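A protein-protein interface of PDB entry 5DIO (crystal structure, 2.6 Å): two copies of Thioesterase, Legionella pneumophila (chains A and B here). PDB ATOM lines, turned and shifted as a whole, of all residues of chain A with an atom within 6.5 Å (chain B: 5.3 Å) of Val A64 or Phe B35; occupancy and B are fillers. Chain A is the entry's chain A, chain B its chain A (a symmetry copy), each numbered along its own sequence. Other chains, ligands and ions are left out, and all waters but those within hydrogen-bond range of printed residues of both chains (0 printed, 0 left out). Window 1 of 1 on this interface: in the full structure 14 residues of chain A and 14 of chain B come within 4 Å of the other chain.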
ATOM      1  N   ASN A  30     -21.367  26.667  36.563  1.00  0.00           N
ATOM      2  CA  ASN A  30     -21.746  25.817  35.429  1.00  0.00           C
ATOM      3  C   ASN A  30     -20.475  25.162  34.908  1.00  0.00           C
ATOM      4  O   ASN A  30     -19.416  25.725  35.045  1.00  0.00           O
ATOM      5  CB  ASN A  30     -22.432  26.675  34.350  1.00  0.00           C
ATOM      6  CG  ASN A  30     -23.007  25.856  33.205  1.00  0.00           C
ATOM      7  OD1 ASN A  30     -22.297  25.457  32.269  1.00  0.00           O
ATOM      8  ND2 ASN A  30     -24.299  25.619  33.259  1.00  0.00           N
ATOM      9  N   ASN A  31     -20.573  23.983  34.360  1.00  0.00           N
ATOM     10  CA  ASN A  31     -19.380  23.421  33.856  1.00  0.00           C
ATOM     11  C   ASN A  31     -19.000  23.807  32.452  1.00  0.00           C
ATOM     12  O   ASN A  31     -17.893  23.609  32.064  1.00  0.00           O
ATOM     13  CB  ASN A  31     -19.186  21.936  34.211  1.00  0.00           C
ATOM     14  CG  ASN A  31     -20.295  21.039  33.740  1.00  0.00           C
ATOM     15  OD1 ASN A  31     -20.604  20.960  32.558  1.00  0.00           O
ATOM     16  ND2 ASN A  31     -20.853  20.293  34.669  1.00  0.00           N
ATOM     17  N   ALA A  32     -19.877  24.424  31.704  1.00  0.00           N
ATOM     18  CA  ALA A  32     -19.417  24.984  30.415  1.00  0.00           C
ATOM     19  C   ALA A  32     -18.472  26.153  30.618  1.00  0.00           C
ATOM     20  O   ALA A  32     -17.578  26.350  29.794  1.00  0.00           O
ATOM     21  CB  ALA A  32     -20.575  25.416  29.553  1.00  0.00           C
ATOM     22  N   PHE A  35     -14.566  25.914  30.637  1.00  0.00           N
ATOM     23  CA  PHE A  35     -13.978  26.052  29.306  1.00  0.00           C
ATOM     24  C   PHE A  35     -13.795  27.515  28.857  1.00  0.00           C
ATOM     25  O   PHE A  35     -12.781  27.859  28.232  1.00  0.00           O
ATOM     26  CB  PHE A  35     -14.786  25.227  28.321  1.00  0.00           C
ATOM     27  CG  PHE A  35     -14.821  23.773  28.689  1.00  0.00           C
ATOM     28  CD1 PHE A  35     -13.675  22.981  28.544  1.00  0.00           C
ATOM     29  CD2 PHE A  35     -15.951  23.195  29.246  1.00  0.00           C
ATOM     30  CE1 PHE A  35     -13.669  21.635  28.917  1.00  0.00           C
ATOM     31  CE2 PHE A  35     -15.962  21.844  29.592  1.00  0.00           C
ATOM     32  CZ  PHE A  35     -14.820  21.062  29.434  1.00  0.00           C
ATOM     33  N   PHE A  38     -10.553  28.310  30.727  1.00  0.00           N
ATOM     34  CA  PHE A  38      -9.361  27.758  30.034  1.00  0.00           C
ATOM     35  C   PHE A  38      -9.113  28.451  28.705  1.00  0.00           C
ATOM     36  O   PHE A  38      -7.979  28.789  28.353  1.00  0.00           O
ATOM     37  CB  PHE A  38      -9.494  26.262  29.789  1.00  0.00           C
ATOM     38  CG  PHE A  38      -9.737  25.459  31.048  1.00  0.00           C
ATOM     39  CD1 PHE A  38      -9.194  25.857  32.268  1.00  0.00           C
ATOM     40  CD2 PHE A  38     -10.536  24.310  31.007  1.00  0.00           C
ATOM     41  CE1 PHE A  38      -9.411  25.108  33.408  1.00  0.00           C
ATOM     42  CE2 PHE A  38     -10.766  23.558  32.153  1.00  0.00           C
ATOM     43  CZ  PHE A  38     -10.188  23.946  33.355  1.00  0.00           C
ATOM     44  N   ARG A  42      -5.531  30.365  27.876  1.00  0.00           N
ATOM     45  CA  ARG A  42      -4.856  29.991  26.660  1.00  0.00           C
ATOM     46  C   ARG A  42      -4.633  31.177  25.700  1.00  0.00           C
ATOM     47  O   ARG A  42      -3.533  31.330  25.168  1.00  0.00           O
ATOM     48  CB  ARG A  42      -5.684  28.898  26.024  1.00  0.00           C
ATOM     49  CG  ARG A  42      -5.236  28.457  24.679  1.00  0.00           C
ATOM     50  CD  ARG A  42      -5.970  27.165  24.360  1.00  0.00           C
ATOM     51  NE  ARG A  42      -7.369  27.389  24.007  1.00  0.00           N
ATOM     52  CZ  ARG A  42      -8.414  26.713  24.467  1.00  0.00           C
ATOM     53  NH1 ARG A  42      -8.285  25.723  25.369  1.00  0.00           N
ATOM     54  NH2 ARG A  42      -9.612  27.042  23.999  1.00  0.00           N
ATOM     55  N   VAL A  61      -8.687  24.714  18.338  1.00  0.00           N
ATOM     56  CA  VAL A  61      -8.931  23.653  19.299  1.00  0.00           C
ATOM     57  C   VAL A  61      -9.638  22.453  18.698  1.00  0.00           C
ATOM     58  O   VAL A  61     -10.733  22.592  18.214  1.00  0.00           O
ATOM     59  CB  VAL A  61      -9.809  24.168  20.429  1.00  0.00           C
ATOM     60  CG1 VAL A  61     -10.191  23.017  21.358  1.00  0.00           C
ATOM     61  CG2 VAL A  61      -9.073  25.261  21.174  1.00  0.00           C
ATOM     62  N   ILE A  62      -9.031  21.275  18.767  1.00  0.00           N
ATOM     63  CA  ILE A  62      -9.621  20.086  18.183  1.00  0.00           C
ATOM     64  C   ILE A  62     -10.272  19.300  19.293  1.00  0.00           C
ATOM     65  O   ILE A  62     -11.180  18.502  19.036  1.00  0.00           O
ATOM     66  CB  ILE A  62      -8.603  19.236  17.358  1.00  0.00           C
ATOM     67  CG1 ILE A  62      -9.074  17.787  17.119  1.00  0.00           C
ATOM     68  CG2 ILE A  62      -7.265  19.079  18.040  1.00  0.00           C
ATOM     69  CD1 ILE A  62     -10.365  17.630  16.305  1.00  0.00           C
ATOM     70  N   HIS A  63      -9.850  19.519  20.536  1.00  0.00           N
ATOM     71  CA  HIS A  63     -10.365  18.714  21.645  1.00  0.00           C
ATOM     72  C   HIS A  63     -10.203  19.475  22.909  1.00  0.00           C
ATOM     73  O   HIS A  63      -9.249  20.211  23.101  1.00  0.00           O
ATOM     74  CB  HIS A  63      -9.586  17.404  21.801  1.00  0.00           C
ATOM     75  CG  HIS A  63     -10.128  16.501  22.869  1.00  0.00           C
ATOM     76  ND1 HIS A  63     -11.172  15.622  22.639  1.00  0.00           N
ATOM     77  CD2 HIS A  63      -9.780  16.335  24.170  1.00  0.00           C
ATOM     78  CE1 HIS A  63     -11.446  14.954  23.754  1.00  0.00           C
ATOM     79  NE2 HIS A  63     -10.620  15.371  24.698  1.00  0.00           N
ATOM     80  N   VAL A  64     -11.106  19.250  23.833  1.00  0.00           N
ATOM     81  CA  VAL A  64     -10.971  19.935  25.098  1.00  0.00           C
ATOM     82  C   VAL A  64     -11.748  19.103  26.098  1.00  0.00           C
ATOM     83  O   VAL A  64     -12.804  18.531  25.771  1.00  0.00           O
ATOM     84  CB  VAL A  64     -11.482  21.394  24.953  1.00  0.00           C
ATOM     85  CG1 VAL A  64     -12.991  21.445  25.079  1.00  0.00           C
ATOM     86  CG2 VAL A  64     -10.843  22.313  25.973  1.00  0.00           C
ATOM     87  N   ALA A  65     -11.190  19.004  27.300  1.00  0.00           N
ATOM     88  CA  ALA A  65     -11.746  18.162  28.361  1.00  0.00           C
ATOM     89  C   ALA A  65     -11.498  18.762  29.711  1.00  0.00           C
ATOM     90  O   ALA A  65     -10.633  19.621  29.857  1.00  0.00           O
ATOM     91  CB  ALA A  65     -11.130  16.778  28.308  1.00  0.00           C
ATOM     92  N   CYS A  66     -12.277  18.331  30.695  1.00  0.00           N
ATOM     93  CA  CYS A  66     -12.101  18.784  32.067  1.00  0.00           C
ATOM     94  C   CYS A  66     -12.670  17.779  33.039  1.00  0.00           C
ATOM     95  O   CYS A  66     -13.776  17.203  32.863  1.00  0.00           O
ATOM     96  CB  CYS A  66     -12.776  20.119  32.292  1.00  0.00           C
ATOM     97  SG  CYS A  66     -12.617  20.798  33.970  1.00  0.00           S
ATOM     98  N   HIS A  96      -4.438  22.437  31.996  1.00  0.00           N
ATOM     99  CA  HIS A  96      -4.754  23.512  32.936  1.00  0.00           C
ATOM    100  C   HIS A  96      -5.156  22.978  34.332  1.00  0.00           C
ATOM    101  O   HIS A  96      -6.070  22.177  34.455  1.00  0.00           O
ATOM    102  CB  HIS A  96      -5.902  24.370  32.382  1.00  0.00           C
ATOM    103  CG  HIS A  96      -5.803  24.675  30.917  1.00  0.00           C
ATOM    104  ND1 HIS A  96      -5.095  25.752  30.425  1.00  0.00           N
ATOM    105  CD2 HIS A  96      -6.355  24.065  29.838  1.00  0.00           C
ATOM    106  CE1 HIS A  96      -5.198  25.780  29.104  1.00  0.00           C
ATOM    107  NE2 HIS A  96      -5.955  24.766  28.722  1.00  0.00           N
ATOM    108  N   VAL A 109      -7.790  20.026  29.983  1.00  0.00           N
ATOM    109  CA  VAL A 109      -6.877  19.637  28.910  1.00  0.00           C
ATOM    110  C   VAL A 109      -7.372  20.228  27.621  1.00  0.00           C
ATOM    111  O   VAL A 109      -8.557  20.125  27.319  1.00  0.00           O
ATOM    112  CB  VAL A 109      -6.877  18.114  28.702  1.00  0.00           C
ATOM    113  CG1 VAL A 109      -6.071  17.760  27.453  1.00  0.00           C
ATOM    114  CG2 VAL A 109      -6.335  17.392  29.947  1.00  0.00           C
ATOM    115  N   SER A 110      -6.491  20.812  26.822  1.00  0.00           N
ATOM    116  CA  SER A 110      -6.932  21.222  25.501  1.00  0.00           C
ATOM    117  C   SER A 110      -5.884  20.992  24.428  1.00  0.00           C
ATOM    118  O   SER A 110      -4.768  21.457  24.536  1.00  0.00           O
ATOM    119  CB  SER A 110      -7.435  22.666  25.539  1.00  0.00           C
ATOM    120  OG  SER A 110      -6.395  23.608  25.527  1.00  0.00           O
ATOM    121  N   LYS A 111      -6.267  20.243  23.400  1.00  0.00           N
ATOM    122  CA  LYS A 111      -5.424  20.005  22.241  1.00  0.00           C
ATOM    123  C   LYS A 111      -5.683  21.098  21.225  1.00  0.00           C
ATOM    124  O   LYS A 111      -6.814  21.348  20.844  1.00  0.00           O
ATOM    125  CB  LYS A 111      -5.696  18.632  21.615  1.00  0.00           C
ATOM    126  CG  LYS A 111      -4.637  18.240  20.583  1.00  0.00           C
ATOM    127  CD  LYS A 111      -4.711  16.782  20.136  1.00  0.00           C
ATOM    128  CE  LYS A 111      -3.571  16.430  19.178  1.00  0.00           C
ATOM    129  NZ  LYS A 111      -3.575  14.975  18.848  1.00  0.00           N
ATOM    130  N   ASN B  31     -16.654  27.148  21.789  1.00  0.00           N
ATOM    131  CA  ASN B  31     -16.645  25.794  22.185  1.00  0.00           C
ATOM    132  C   ASN B  31     -17.086  25.507  23.595  1.00  0.00           C
ATOM    133  O   ASN B  31     -17.372  24.395  23.909  1.00  0.00           O
ATOM    134  CB  ASN B  31     -15.413  25.007  21.703  1.00  0.00           C
ATOM    135  CG  ASN B  31     -14.100  25.579  22.155  1.00  0.00           C
ATOM    136  OD1 ASN B  31     -13.834  25.727  23.341  1.00  0.00           O
ATOM    137  ND2 ASN B  31     -13.233  25.832  21.198  1.00  0.00           N
ATOM    138  N   ALA B  32     -17.220  26.500  24.434  1.00  0.00           N
ATOM    139  CA  ALA B  32     -17.859  26.225  25.738  1.00  0.00           C
ATOM    140  C   ALA B  32     -19.331  25.897  25.582  1.00  0.00           C
ATOM    141  O   ALA B  32     -19.857  25.112  26.374  1.00  0.00           O
ATOM    142  CB  ALA B  32     -17.698  27.382  26.690  1.00  0.00           C
ATOM    143  N   ARG B  33     -19.977  26.476  24.554  1.00  0.00           N
ATOM    144  CA  ARG B  33     -21.429  26.362  24.359  1.00  0.00           C
ATOM    145  C   ARG B  33     -21.827  24.991  24.002  1.00  0.00           C
ATOM    146  O   ARG B  33     -22.964  24.595  24.296  1.00  0.00           O
ATOM    147  CB  ARG B  33     -21.938  27.328  23.291  1.00  0.00           C
ATOM    148  CG  ARG B  33     -21.902  28.795  23.744  1.00  0.00           C
ATOM    149  CD  ARG B  33     -22.973  29.066  24.789  1.00  0.00           C
ATOM    150  NE  ARG B  33     -24.302  28.641  24.303  1.00  0.00           N
ATOM    151  CZ  ARG B  33     -25.348  28.319  25.072  1.00  0.00           C
ATOM    152  NH1 ARG B  33     -25.262  28.356  26.401  1.00  0.00           N
ATOM    153  NH2 ARG B  33     -26.500  27.958  24.513  1.00  0.00           N
ATOM    154  N   TYR B  34     -20.912  24.244  23.396  1.00  0.00           N
ATOM    155  CA  TYR B  34     -21.188  22.842  23.045  1.00  0.00           C
ATOM    156  C   TYR B  34     -21.580  22.070  24.289  1.00  0.00           C
ATOM    157  O   TYR B  34     -22.574  21.340  24.302  1.00  0.00           O
ATOM    158  CB  TYR B  34     -19.989  22.188  22.413  1.00  0.00           C
ATOM    159  CG  TYR B  34     -19.758  22.560  20.980  1.00  0.00           C
ATOM    160  CD1 TYR B  34     -19.173  23.776  20.632  1.00  0.00           C
ATOM    161  CD2 TYR B  34     -20.037  21.671  19.957  1.00  0.00           C
ATOM    162  CE1 TYR B  34     -18.911  24.098  19.302  1.00  0.00           C
ATOM    163  CE2 TYR B  34     -19.761  21.985  18.619  1.00  0.00           C
ATOM    164  CZ  TYR B  34     -19.200  23.190  18.310  1.00  0.00           C
ATOM    165  OH  TYR B  34     -18.971  23.472  16.988  1.00  0.00           O
ATOM    166  N   PHE B  35     -20.822  22.286  25.347  1.00  0.00           N
ATOM    167  CA  PHE B  35     -21.134  21.710  26.654  1.00  0.00           C
ATOM    168  C   PHE B  35     -22.506  22.140  27.209  1.00  0.00           C
ATOM    169  O   PHE B  35     -23.226  21.328  27.808  1.00  0.00           O
ATOM    170  CB  PHE B  35     -19.991  22.001  27.608  1.00  0.00           C
ATOM    171  CG  PHE B  35     -18.688  21.434  27.128  1.00  0.00           C
ATOM    172  CD1 PHE B  35     -18.469  20.051  27.150  1.00  0.00           C
ATOM    173  CD2 PHE B  35     -17.704  22.245  26.583  1.00  0.00           C
ATOM    174  CE1 PHE B  35     -17.281  19.494  26.670  1.00  0.00           C
ATOM    175  CE2 PHE B  35     -16.503  21.699  26.131  1.00  0.00           C
ATOM    176  CZ  PHE B  35     -16.291  20.322  26.167  1.00  0.00           C
ATOM    177  N   ASP B  36     -22.898  23.383  26.953  1.00  0.00           N
ATOM    178  CA  ASP B  36     -24.288  23.798  27.180  1.00  0.00           C
ATOM    179  C   ASP B  36     -25.262  22.949  26.382  1.00  0.00           C
ATOM    180  O   ASP B  36     -26.285  22.500  26.917  1.00  0.00           O
ATOM    181  CB  ASP B  36     -24.472  25.303  26.907  1.00  0.00           C
ATOM    182  CG  ASP B  36     -23.666  26.184  27.894  1.00  0.00           C
ATOM    183  OD1 ASP B  36     -23.320  25.687  28.973  1.00  0.00           O
ATOM    184  OD2 ASP B  36     -23.371  27.358  27.631  1.00  0.00           O
ATOM    185  N   TYR B  37     -24.954  22.647  25.131  1.00  0.00           N
ATOM    186  CA  TYR B  37     -25.857  21.736  24.398  1.00  0.00           C
ATOM    187  C   TYR B  37     -25.887  20.309  24.941  1.00  0.00           C
ATOM    188  O   TYR B  37     -26.977  19.746  25.092  1.00  0.00           O
ATOM    189  CB  TYR B  37     -25.568  21.681  22.903  1.00  0.00           C
ATOM    190  CG  TYR B  37     -25.433  23.011  22.215  1.00  0.00           C
ATOM    191  CD1 TYR B  37     -26.279  24.060  22.517  1.00  0.00           C
ATOM    192  CD2 TYR B  37     -24.473  23.198  21.225  1.00  0.00           C
ATOM    193  CE1 TYR B  37     -26.162  25.264  21.876  1.00  0.00           C
ATOM    194  CE2 TYR B  37     -24.348  24.401  20.580  1.00  0.00           C
ATOM    195  CZ  TYR B  37     -25.201  25.426  20.925  1.00  0.00           C
ATOM    196  OH  TYR B  37     -25.092  26.628  20.276  1.00  0.00           O
ATOM    197  N   PHE B  38     -24.728  19.721  25.248  1.00  0.00           N
ATOM    198  CA  PHE B  38     -24.717  18.356  25.833  1.00  0.00           C
ATOM    199  C   PHE B  38     -25.382  18.326  27.199  1.00  0.00           C
ATOM    200  O   PHE B  38     -26.162  17.424  27.520  1.00  0.00           O
ATOM    201  CB  PHE B  38     -23.303  17.811  25.963  1.00  0.00           C
ATOM    202  CG  PHE B  38     -22.539  17.783  24.657  1.00  0.00           C
ATOM    203  CD1 PHE B  38     -23.195  17.565  23.447  1.00  0.00           C
ATOM    204  CD2 PHE B  38     -21.156  18.002  24.646  1.00  0.00           C
ATOM    205  CE1 PHE B  38     -22.485  17.529  22.264  1.00  0.00           C
ATOM    206  CE2 PHE B  38     -20.438  17.977  23.457  1.00  0.00           C
ATOM    207  CZ  PHE B  38     -21.099  17.721  22.262  1.00  0.00           C
ATOM    208  N   GLN B  39     -25.093  19.341  27.997  1.00  0.00           N
ATOM    209  CA  GLN B  39     -25.782  19.489  29.241  1.00  0.00           C
ATOM    210  C   GLN B  39     -27.331  19.472  29.074  1.00  0.00           C
ATOM    211  O   GLN B  39     -28.006  18.853  29.886  1.00  0.00           O
ATOM    212  CB  GLN B  39     -25.293  20.758  29.914  1.00  0.00           C
ATOM    213  CG  GLN B  39     -26.024  21.104  31.188  1.00  0.00           C
ATOM    214  CD  GLN B  39     -25.535  22.417  31.735  1.00  0.00           C
ATOM    215  OE1 GLN B  39     -24.477  22.468  32.352  1.00  0.00           O
ATOM    216  NE2 GLN B  39     -26.279  23.498  31.473  1.00  0.00           N
ATOM    217  N   GLU B  40     -27.882  20.129  28.043  1.00  0.00           N
ATOM    218  CA  GLU B  40     -29.357  20.170  27.858  1.00  0.00           C
ATOM    219  C   GLU B  40     -29.928  18.846  27.370  1.00  0.00           C
ATOM    220  O   GLU B  40     -31.091  18.509  27.640  1.00  0.00           O
ATOM    221  CB  GLU B  40     -29.795  21.262  26.850  1.00  0.00           C
ATOM    222  CG  GLU B  40     -29.819  22.712  27.347  1.00  0.00           C
ATOM    223  CD  GLU B  40     -30.583  22.879  28.646  1.00  0.00           C
ATOM    224  OE1 GLU B  40     -31.750  22.391  28.738  1.00  0.00           O
ATOM    225  OE2 GLU B  40     -30.002  23.483  29.583  1.00  0.00           O
ATOM    226  N   VAL B  64     -16.000  15.753  31.409  1.00  0.00           N
ATOM    227  CA  VAL B  64     -16.737  16.030  30.199  1.00  0.00           C
ATOM    228  C   VAL B  64     -15.702  16.449  29.175  1.00  0.00           C
ATOM    229  O   VAL B  64     -14.710  17.124  29.508  1.00  0.00           O
ATOM    230  CB  VAL B  64     -17.818  17.107  30.486  1.00  0.00           C
ATOM    231  CG1 VAL B  64     -17.213  18.494  30.440  1.00  0.00           C
ATOM    232  CG2 VAL B  64     -18.974  17.011  29.512  1.00  0.00           C
ATOM    233  N   ALA B  65     -15.916  16.001  27.943  1.00  0.00           N
ATOM    234  CA  ALA B  65     -14.971  16.224  26.847  1.00  0.00           C
ATOM    235  C   ALA B  65     -15.687  16.368  25.538  1.00  0.00           C
ATOM    236  O   ALA B  65     -16.843  15.973  25.419  1.00  0.00           O
ATOM    237  CB  ALA B  65     -13.994  15.068  26.757  1.00  0.00           C
ATOM    238  N   CYS B  66     -15.009  16.961  24.564  1.00  0.00           N
ATOM    239  CA  CYS B  66     -15.562  17.108  23.226  1.00  0.00           C
ATOM    240  C   CYS B  66     -14.461  17.265  22.205  1.00  0.00           C
ATOM    241  O   CYS B  66     -13.452  17.995  22.390  1.00  0.00           O
ATOM    242  CB  CYS B  66     -16.479  18.309  23.143  1.00  0.00           C
ATOM    243  SG  CYS B  66     -17.243  18.595  21.519  1.00  0.00           S
ATOM    244  N   THR B  67     -14.676  16.551  21.119  1.00  0.00           N
ATOM    245  CA  THR B  67     -13.820  16.602  19.951  1.00  0.00           C
ATOM    246  C   THR B  67     -14.557  17.413  18.880  1.00  0.00           C
ATOM    247  O   THR B  67     -15.746  17.188  18.635  1.00  0.00           O
ATOM    248  CB  THR B  67     -13.487  15.151  19.538  1.00  0.00           C
ATOM    249  OG1 THR B  67     -12.816  14.512  20.659  1.00  0.00           O
ATOM    250  CG2 THR B  67     -12.606  15.108  18.309  1.00  0.00           C
ATOM    251  N   PHE B  68     -13.878  18.407  18.312  1.00  0.00           N
ATOM    252  CA  PHE B  68     -14.510  19.321  17.357  1.00  0.00           C
ATOM    253  C   PHE B  68     -14.086  18.963  15.946  1.00  0.00           C
ATOM    254  O   PHE B  68     -12.983  19.328  15.522  1.00  0.00           O
ATOM    255  CB  PHE B  68     -14.129  20.772  17.686  1.00  0.00           C
ATOM    256  CG  PHE B  68     -14.479  21.164  19.080  1.00  0.00           C
ATOM    257  CD1 PHE B  68     -15.766  21.486  19.418  1.00  0.00           C
ATOM    258  CD2 PHE B  68     -13.529  21.173  20.067  1.00  0.00           C
ATOM    259  CE1 PHE B  68     -16.090  21.835  20.718  1.00  0.00           C
ATOM    260  CE2 PHE B  68     -13.841  21.520  21.371  1.00  0.00           C
ATOM    261  CZ  PHE B  68     -15.128  21.847  21.697  1.00  0.00           C
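Of the 16 printed residues of chain A, 9 touch a printed residue of chain B.
Printed residues of chain A that touch a printed residue of chain B: Asn A30, Ala A32, Phe A35, Val A61, Ile A62, His A63, Val A64, Ala A65 and Cys A66.
Among the printed residues, 22 pairs touch across the chains.
Among the printed residues, no Asp or Glu carboxylate lies within 4 Å of a Lys or Arg side-chain nitrogen of the other chain.
Ala A32 touches Ala B32.
Ala A32 touches Asp B36 (CB to OD1, 2.8 Å).
CB of Phe A35 touches CB of Ala B32, 3.97 Å away.
Phe B35 touches Phe A35.
Val B64 touches Phe A35 (CG1 to CZ, 3.7 Å).
Val A61 touches Asn B31 (CB to ND2, 3.9 Å).
Thr B67 touches Ile A62.
Ala B65 touches His A63 (CB to CE1, 3.9 Å).
Val A64 touches Phe B35.
Ala B65 touches Val A64.
Phe A35 touches its own counterpart, Phe B35.
Phe A35 touches Val B64, and with the chains exchanged Val A64 touches Phe B35.
Val A64 touches Cys B66, and with the chains exchanged Cys A66 touches Val B64.
Ala B65 touches its own counterpart, Ala A65.
N of Ile A62 sits at hydrogen-bond distance from O of Lys A111.
The side-chain carboxylate (OD2) of Asp B36 lies within salt-bridge range of the guanidinium group (NH1) of Arg B33, at 2.5 Å.
The backbone NH of Lys A111 lies within hydrogen-bond range of the backbone carbonyl oxygen of His A63 (3.0 Å).
N of Ala A32 sits at hydrogen-bond distance from OD1 of Asn A30, 2.7 Å away.
The backbone NH (N) of Ala A65 sits at hydrogen-bond distance from the backbone carbonyl oxygen (O) of Val A109 (2.9 Å).
Of chain B, only Phe B35 (3.7 Å), Ala B65 (3.3 Å), Cys B66 (3.0 Å) and Phe B68 (3.8 Å) come within 4 Å of Val A64.
Of the printed residues of chain B, Ala A65 touches Val B64 and Ala B65.
Of the printed residues of chain A, Ala B32 touches Ala A32 (3.3 Å) and Phe A35 (3.97 Å).
Tyr B34 touches none of the printed residues of chain A.
Phe B35 touches three residues of chain A.
Of the printed residues of chain A, Ala B65 touches His A63 (3.9 Å), Val A64 (3.3 Å) and Ala A65 (3.7 Å).
Printed residues of chain A within 4 Å of Cys B66: His A63 and Val A64.
The nearest residue of chain B that does not touch Val A64 is Val B64 (4.4 Å).
The nearest printed residue of chain B that does not touch Ala A32 is Gln B39 (5.0 Å).
OG1 of Thr B67 is in hydrogen-bond range of ND1 of His A63 (2.8 Å).
The backbone carbonyl oxygen (O) of Val A64 is in hydrogen-bond range of the backbone NH (N) of Cys B66.
The side-chain carboxylate (OD1) of Asp B36 sits close to the side-chain amide oxygen (OD1) of Asn A30 (3.5 Å).
The side-chain amide nitrogen (ND2) of Asn A30 sits at hydrogen-bond distance from the side-chain amide oxygen (OE1) of Gln B39 (3.3 Å).
A ring nitrogen (ND1) of His A63 sits close to the backbone carbonyl oxygen (O) of Cys B66, 3.3 Å away.
The backbone NH of Cys A66 is in hydrogen-bond range of the backbone carbonyl oxygen of Val B64, at 3.0 Å.
O of Ile A62 lies within hydrogen-bond range of N of Phe B68 (2.8 Å).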
